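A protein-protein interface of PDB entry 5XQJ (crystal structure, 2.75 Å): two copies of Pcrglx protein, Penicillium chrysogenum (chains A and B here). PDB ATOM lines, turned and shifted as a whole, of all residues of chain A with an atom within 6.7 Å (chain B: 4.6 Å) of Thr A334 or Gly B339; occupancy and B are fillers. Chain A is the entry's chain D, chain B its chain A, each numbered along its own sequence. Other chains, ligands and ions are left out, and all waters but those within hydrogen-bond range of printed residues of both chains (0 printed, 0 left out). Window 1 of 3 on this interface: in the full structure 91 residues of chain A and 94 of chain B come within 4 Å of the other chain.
Gly A337 touches its own counterpart, Gly B337. Positions printed for both chains: 331, 337 and 338.
Thr A334 touches just these residues of chain B: Gly B337, Phe B338 and Gly B339. Printed residues of chain A within 4 Å of Gly B339: Thr A334 (3.7 Å). Of the printed residues of chain A, Gly B337 touches Thr A334 (3.5 Å), Asp A336 (3.7 Å) and Gly A337 (3.9 Å). Printed residues of chain A within 4 Å of Phe B338: Thr A334. Of the printed residues of chain B, Asp A336 touches Gly B337. Printed residues of chain B within 4 Å of Gly A337: Gly B337 (3.9 Å). Ala A335 touches none of the printed residues of chain B.
The backbone carbonyl oxygen (O) of Thr B331 lies within hydrogen-bond range of the backbone NH (N) of Gly B339. NE2 of Gln A332 sits at hydrogen-bond distance from O of Gly A337 (3.1 Å). The backbone carbonyl oxygen of Thr A334 sits at hydrogen-bond distance from the side-chain amide nitrogen of Gln A332, at 2.9 Å. The backbone NH (N) of Gly A337 lies close to the backbone carbonyl oxygen (O) of Thr A357 (3.2 Å). The backbone carbonyl oxygen (O) of Phe B338 sits close to the side-chain hydroxyl (OG) of Ser B355 (3.4 Å). The side-chain hydroxyl (OG1) of Thr A334 is in hydrogen-bond range of the backbone NH (N) of Gly A337, at 3.0 Å.
Among the printed residues, pairs that only touch across the chains: Thr A334 with Gly B337, Thr A334 with Phe B338, Thr A334 with Gly B339, Asp A336 with Gly B337 and Gly A337 with Gly B337.
Among the printed residues, no Asp or Glu carboxylate lies within 4 Å of a Lys or Arg side-chain nitrogen of the other chain.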
ATOM      1  N   THR A 331     -30.603  -1.543  13.845  1.00  0.00           N
ATOM      2  CA  THR A 331     -29.855  -1.055  12.674  1.00  0.00           C
ATOM      3  C   THR A 331     -29.986  -2.051  11.516  1.00  0.00           C
ATOM      4  O   THR A 331     -29.614  -3.214  11.646  1.00  0.00           O
ATOM      5  CB  THR A 331     -28.357  -0.861  13.020  1.00  0.00           C
ATOM      6  OG1 THR A 331     -27.924  -1.886  13.922  1.00  0.00           O
ATOM      7  CG2 THR A 331     -28.150   0.484  13.707  1.00  0.00           C
ATOM      8  N   GLN A 332     -30.529  -1.593  10.386  1.00  0.00           N
ATOM      9  CA  GLN A 332     -30.642  -2.404   9.184  1.00  0.00           C
ATOM     10  C   GLN A 332     -29.646  -1.860   8.150  1.00  0.00           C
ATOM     11  O   GLN A 332     -29.956  -0.935   7.462  1.00  0.00           O
ATOM     12  CB  GLN A 332     -32.066  -2.348   8.689  1.00  0.00           C
ATOM     13  CG  GLN A 332     -32.363  -3.186   7.436  1.00  0.00           C
ATOM     14  CD  GLN A 332     -32.631  -4.637   7.758  1.00  0.00           C
ATOM     15  OE1 GLN A 332     -33.530  -4.948   8.551  1.00  0.00           O
ATOM     16  NE2 GLN A 332     -31.847  -5.535   7.166  1.00  0.00           N
ATOM     17  N   LEU A 333     -28.444  -2.445   8.069  1.00  0.00           N
ATOM     18  CA  LEU A 333     -27.295  -1.891   7.299  1.00  0.00           C
ATOM     19  C   LEU A 333     -27.063  -2.571   5.950  1.00  0.00           C
ATOM     20  O   LEU A 333     -26.411  -2.024   5.107  1.00  0.00           O
ATOM     21  CB  LEU A 333     -26.005  -1.946   8.146  1.00  0.00           C
ATOM     22  CG  LEU A 333     -26.026  -1.275   9.555  1.00  0.00           C
ATOM     23  CD1 LEU A 333     -24.628  -1.090  10.204  1.00  0.00           C
ATOM     24  CD2 LEU A 333     -26.777   0.053   9.520  1.00  0.00           C
ATOM     25  N   THR A 334     -27.591  -3.770   5.782  1.00  0.00           N
ATOM     26  CA  THR A 334     -27.705  -4.434   4.487  1.00  0.00           C
ATOM     27  C   THR A 334     -29.199  -4.653   4.249  1.00  0.00           C
ATOM     28  O   THR A 334     -30.009  -4.455   5.146  1.00  0.00           O
ATOM     29  CB  THR A 334     -26.964  -5.803   4.465  1.00  0.00           C
ATOM     30  OG1 THR A 334     -27.311  -6.592   5.614  1.00  0.00           O
ATOM     31  CG2 THR A 334     -25.454  -5.637   4.471  1.00  0.00           C
ATOM     32  N   ALA A 335     -29.560  -5.040   3.042  1.00  0.00           N
ATOM     33  CA  ALA A 335     -30.914  -5.582   2.808  1.00  0.00           C
ATOM     34  C   ALA A 335     -31.169  -6.953   3.480  1.00  0.00           C
ATOM     35  O   ALA A 335     -32.300  -7.384   3.576  1.00  0.00           O
ATOM     36  CB  ALA A 335     -31.177  -5.708   1.307  1.00  0.00           C
ATOM     37  N   ASP A 336     -30.111  -7.621   3.945  1.00  0.00           N
ATOM     38  CA  ASP A 336     -30.200  -8.973   4.441  1.00  0.00           C
ATOM     39  C   ASP A 336     -30.060  -9.191   5.934  1.00  0.00           C
ATOM     40  O   ASP A 336     -30.488 -10.235   6.396  1.00  0.00           O
ATOM     41  CB  ASP A 336     -29.190  -9.822   3.705  1.00  0.00           C
ATOM     42  CG  ASP A 336     -29.495  -9.901   2.247  1.00  0.00           C
ATOM     43  OD1 ASP A 336     -30.548 -10.492   1.917  1.00  0.00           O
ATOM     44  OD2 ASP A 336     -28.710  -9.352   1.444  1.00  0.00           O
ATOM     45  N   GLY A 337     -29.537  -8.232   6.692  1.00  0.00           N
ATOM     46  CA  GLY A 337     -29.325  -8.458   8.113  1.00  0.00           C
ATOM     47  C   GLY A 337     -29.545  -7.262   9.001  1.00  0.00           C
ATOM     48  O   GLY A 337     -29.203  -6.146   8.614  1.00  0.00           O
ATOM     49  N   PHE A 338     -30.089  -7.476  10.208  1.00  0.00           N
ATOM     50  CA  PHE A 338     -30.156  -6.382  11.189  1.00  0.00           C
ATOM     51  C   PHE A 338     -29.610  -6.747  12.558  1.00  0.00           C
ATOM     52  O   PHE A 338     -29.722  -7.890  13.001  1.00  0.00           O
ATOM     53  CB  PHE A 338     -31.570  -5.754  11.314  1.00  0.00           C
ATOM     54  CG  PHE A 338     -32.588  -6.613  11.994  1.00  0.00           C
ATOM     55  CD1 PHE A 338     -33.328  -7.539  11.273  1.00  0.00           C
ATOM     56  CD2 PHE A 338     -32.857  -6.467  13.354  1.00  0.00           C
ATOM     57  CE1 PHE A 338     -34.299  -8.336  11.905  1.00  0.00           C
ATOM     58  CE2 PHE A 338     -33.831  -7.268  13.993  1.00  0.00           C
ATOM     59  CZ  PHE A 338     -34.546  -8.199  13.268  1.00  0.00           C
ATOM     60  N   THR A 357     -32.925 -11.217  10.103  1.00  0.00           N
ATOM     61  CA  THR A 357     -32.609 -10.860   8.721  1.00  0.00           C
ATOM     62  C   THR A 357     -33.119  -9.487   8.329  1.00  0.00           C
ATOM     63  O   THR A 357     -32.362  -8.578   8.085  1.00  0.00           O
ATOM     64  CB  THR A 357     -33.241 -11.891   7.780  1.00  0.00           C
ATOM     65  OG1 THR A 357     -34.643 -11.944   8.038  1.00  0.00           O
ATOM     66  CG2 THR A 357     -32.660 -13.271   8.046  1.00  0.00           C
ATOM     67  N   ARG A 358     -34.441  -9.370   8.309  1.00  0.00           N
ATOM     68  CA  ARG A 358     -35.166  -8.252   7.707  1.00  0.00           C
ATOM     69  C   ARG A 358     -36.282  -7.749   8.621  1.00  0.00           C
ATOM     70  O   ARG A 358     -37.361  -8.331   8.677  1.00  0.00           O
ATOM     71  CB  ARG A 358     -35.769  -8.713   6.383  1.00  0.00           C
ATOM     72  CG  ARG A 358     -34.716  -8.837   5.320  1.00  0.00           C
ATOM     73  CD  ARG A 358     -35.240  -9.460   4.048  1.00  0.00           C
ATOM     74  NE  ARG A 358     -34.167  -9.588   3.056  1.00  0.00           N
ATOM     75  CZ  ARG A 358     -34.334 -10.067   1.837  1.00  0.00           C
ATOM     76  NH1 ARG A 358     -35.521 -10.469   1.438  1.00  0.00           N
ATOM     77  NH2 ARG A 358     -33.299 -10.158   1.005  1.00  0.00           N
ATOM     78  N   TRP A 381     -36.439  -2.268   5.158  1.00  0.00           N
ATOM     79  CA  TRP A 381     -35.199  -3.005   4.841  1.00  0.00           C
ATOM     80  C   TRP A 381     -34.847  -2.914   3.356  1.00  0.00           C
ATOM     81  O   TRP A 381     -33.690  -3.053   3.001  1.00  0.00           O
ATOM     82  CB  TRP A 381     -35.232  -4.491   5.346  1.00  0.00           C
ATOM     83  CG  TRP A 381     -36.358  -5.338   4.737  1.00  0.00           C
ATOM     84  CD1 TRP A 381     -37.565  -5.595   5.292  1.00  0.00           C
ATOM     85  CD2 TRP A 381     -36.344  -6.004   3.489  1.00  0.00           C
ATOM     86  NE1 TRP A 381     -38.320  -6.383   4.468  1.00  0.00           N
ATOM     87  CE2 TRP A 381     -37.602  -6.639   3.339  1.00  0.00           C
ATOM     88  CE3 TRP A 381     -35.389  -6.140   2.476  1.00  0.00           C
ATOM     89  CZ2 TRP A 381     -37.953  -7.375   2.206  1.00  0.00           C
ATOM     90  CZ3 TRP A 381     -35.719  -6.882   1.348  1.00  0.00           C
ATOM     91  CH2 TRP A 381     -37.013  -7.486   1.216  1.00  0.00           C
ATOM     92  N   LYS A 382     -35.826  -2.650   2.493  1.00  0.00           N
ATOM     93  CA  LYS A 382     -35.548  -2.453   1.077  1.00  0.00           C
ATOM     94  C   LYS A 382     -34.954  -1.087   0.788  1.00  0.00           C
ATOM     95  O   LYS A 382     -34.563  -0.807  -0.329  1.00  0.00           O
ATOM     96  CB  LYS A 382     -36.826  -2.620   0.279  1.00  0.00           C
ATOM     97  CG  LYS A 382     -37.437  -4.035   0.305  1.00  0.00           C
ATOM     98  CD  LYS A 382     -38.958  -4.010   0.160  1.00  0.00           C
ATOM     99  CE  LYS A 382     -39.462  -4.900  -0.965  1.00  0.00           C
ATOM    100  NZ  LYS A 382     -40.946  -4.750  -1.104  1.00  0.00           N
ATOM    101  N   TYR A 384     -32.587   0.361   2.972  1.00  0.00           N
ATOM    102  CA  TYR A 384     -31.416   0.365   3.862  1.00  0.00           C
ATOM    103  C   TYR A 384     -30.348   1.314   3.300  1.00  0.00           C
ATOM    104  O   TYR A 384     -30.245   1.493   2.091  1.00  0.00           O
ATOM    105  CB  TYR A 384     -30.851  -1.107   3.991  1.00  0.00           C
ATOM    106  CG  TYR A 384     -29.944  -1.450   2.845  1.00  0.00           C
ATOM    107  CD1 TYR A 384     -30.458  -1.836   1.637  1.00  0.00           C
ATOM    108  CD2 TYR A 384     -28.572  -1.250   2.949  1.00  0.00           C
ATOM    109  CE1 TYR A 384     -29.639  -2.043   0.551  1.00  0.00           C
ATOM    110  CE2 TYR A 384     -27.732  -1.458   1.878  1.00  0.00           C
ATOM    111  CZ  TYR A 384     -28.271  -1.854   0.668  1.00  0.00           C
ATOM    112  OH  TYR A 384     -27.433  -2.097  -0.420  1.00  0.00           O
ATOM    113  N   PRO A 385     -29.503   1.897   4.133  1.00  0.00           N
ATOM    114  CA  PRO A 385     -29.380   1.624   5.556  1.00  0.00           C
ATOM    115  C   PRO A 385     -30.274   2.492   6.367  1.00  0.00           C
ATOM    116  O   PRO A 385     -30.180   3.696   6.282  1.00  0.00           O
ATOM    117  CB  PRO A 385     -27.937   2.015   5.861  1.00  0.00           C
ATOM    118  CG  PRO A 385     -27.585   3.017   4.823  1.00  0.00           C
ATOM    119  CD  PRO A 385     -28.303   2.551   3.587  1.00  0.00           C
ATOM    120  N   GLY B 329     -14.401  -3.939  -1.182  1.00  0.00           N
ATOM    121  CA  GLY B 329     -14.679  -4.117   0.219  1.00  0.00           C
ATOM    122  C   GLY B 329     -15.909  -4.933   0.511  1.00  0.00           C
ATOM    123  O   GLY B 329     -17.038  -4.524   0.213  1.00  0.00           O
ATOM    124  N   LEU B 330     -15.693  -6.098   1.108  1.00  0.00           N
ATOM    125  CA  LEU B 330     -16.787  -6.933   1.627  1.00  0.00           C
ATOM    126  C   LEU B 330     -16.912  -6.721   3.143  1.00  0.00           C
ATOM    127  O   LEU B 330     -15.896  -6.839   3.863  1.00  0.00           O
ATOM    128  CB  LEU B 330     -16.501  -8.389   1.329  1.00  0.00           C
ATOM    129  CG  LEU B 330     -17.675  -9.380   1.456  1.00  0.00           C
ATOM    130  CD1 LEU B 330     -17.330 -10.644   0.664  1.00  0.00           C
ATOM    131  CD2 LEU B 330     -17.994  -9.715   2.908  1.00  0.00           C
ATOM    132  N   THR B 331     -18.127  -6.422   3.625  1.00  0.00           N
ATOM    133  CA  THR B 331     -18.367  -6.234   5.057  1.00  0.00           C
ATOM    134  C   THR B 331     -19.503  -7.120   5.576  1.00  0.00           C
ATOM    135  O   THR B 331     -20.577  -7.102   5.020  1.00  0.00           O
ATOM    136  CB  THR B 331     -18.662  -4.760   5.380  1.00  0.00           C
ATOM    137  OG1 THR B 331     -19.540  -4.190   4.395  1.00  0.00           O
ATOM    138  CG2 THR B 331     -17.360  -3.970   5.426  1.00  0.00           C
ATOM    139  N   GLY B 337     -26.279 -10.716   7.028  1.00  0.00           N
ATOM    140  CA  GLY B 337     -26.173  -9.945   5.776  1.00  0.00           C
ATOM    141  C   GLY B 337     -24.819  -9.319   5.580  1.00  0.00           C
ATOM    142  O   GLY B 337     -24.236  -8.834   6.538  1.00  0.00           O
ATOM    143  N   PHE B 338     -24.318  -9.321   4.354  1.00  0.00           N
ATOM    144  CA  PHE B 338     -23.026  -8.668   4.056  1.00  0.00           C
ATOM    145  C   PHE B 338     -23.170  -7.671   2.914  1.00  0.00           C
ATOM    146  O   PHE B 338     -24.048  -7.829   2.052  1.00  0.00           O
ATOM    147  CB  PHE B 338     -21.894  -9.706   3.776  1.00  0.00           C
ATOM    148  CG  PHE B 338     -21.993 -10.397   2.438  1.00  0.00           C
ATOM    149  CD1 PHE B 338     -21.376  -9.868   1.310  1.00  0.00           C
ATOM    150  CD2 PHE B 338     -22.691 -11.606   2.310  1.00  0.00           C
ATOM    151  CE1 PHE B 338     -21.484 -10.516   0.068  1.00  0.00           C
ATOM    152  CE2 PHE B 338     -22.789 -12.253   1.078  1.00  0.00           C
ATOM    153  CZ  PHE B 338     -22.190 -11.709  -0.054  1.00  0.00           C
ATOM    154  N   GLY B 339     -22.309  -6.653   2.915  1.00  0.00           N
ATOM    155  CA  GLY B 339     -22.298  -5.645   1.849  1.00  0.00           C
ATOM    156  C   GLY B 339     -21.089  -5.910   1.019  1.00  0.00           C
ATOM    157  O   GLY B 339     -20.199  -6.581   1.475  1.00  0.00           O
ATOM    158  N   LEU B 340     -21.048  -5.399  -0.195  1.00  0.00           N
ATOM    159  CA  LEU B 340     -19.924  -5.628  -1.070  1.00  0.00           C
ATOM    160  C   LEU B 340     -19.858  -4.482  -2.015  1.00  0.00           C
ATOM    161  O   LEU B 340     -20.852  -4.173  -2.649  1.00  0.00           O
ATOM    162  CB  LEU B 340     -20.152  -6.903  -1.849  1.00  0.00           C
ATOM    163  CG  LEU B 340     -19.027  -7.398  -2.765  1.00  0.00           C
ATOM    164  CD1 LEU B 340     -17.694  -7.577  -2.041  1.00  0.00           C
ATOM    165  CD2 LEU B 340     -19.459  -8.718  -3.391  1.00  0.00           C
ATOM    166  N   LYS B 341     -18.699  -3.835  -2.120  1.00  0.00           N
ATOM    167  CA  LYS B 341     -18.556  -2.632  -2.975  1.00  0.00           C
ATOM    168  C   LYS B 341     -17.148  -2.497  -3.541  1.00  0.00           C
ATOM    169  O   LYS B 341     -16.177  -2.956  -2.939  1.00  0.00           O
ATOM    170  CB  LYS B 341     -18.941  -1.365  -2.220  1.00  0.00           C
ATOM    171  CG  LYS B 341     -18.369  -1.314  -0.821  1.00  0.00           C
ATOM    172  CD  LYS B 341     -18.464   0.056  -0.170  1.00  0.00           C
ATOM    173  CE  LYS B 341     -17.325   0.185   0.841  1.00  0.00           C
ATOM    174  NZ  LYS B 341     -17.516   1.334   1.741  1.00  0.00           N
ATOM    175  N   SER B 355     -25.147  -8.239  -3.476  1.00  0.00           N
ATOM    176  CA  SER B 355     -24.564  -8.906  -2.300  1.00  0.00           C
ATOM    177  C   SER B 355     -25.494 -10.033  -1.778  1.00  0.00           C
ATOM    178  O   SER B 355     -26.336 -10.557  -2.519  1.00  0.00           O
ATOM    179  CB  SER B 355     -24.321  -7.830  -1.236  1.00  0.00           C
ATOM    180  OG  SER B 355     -25.567  -7.221  -0.943  1.00  0.00           O
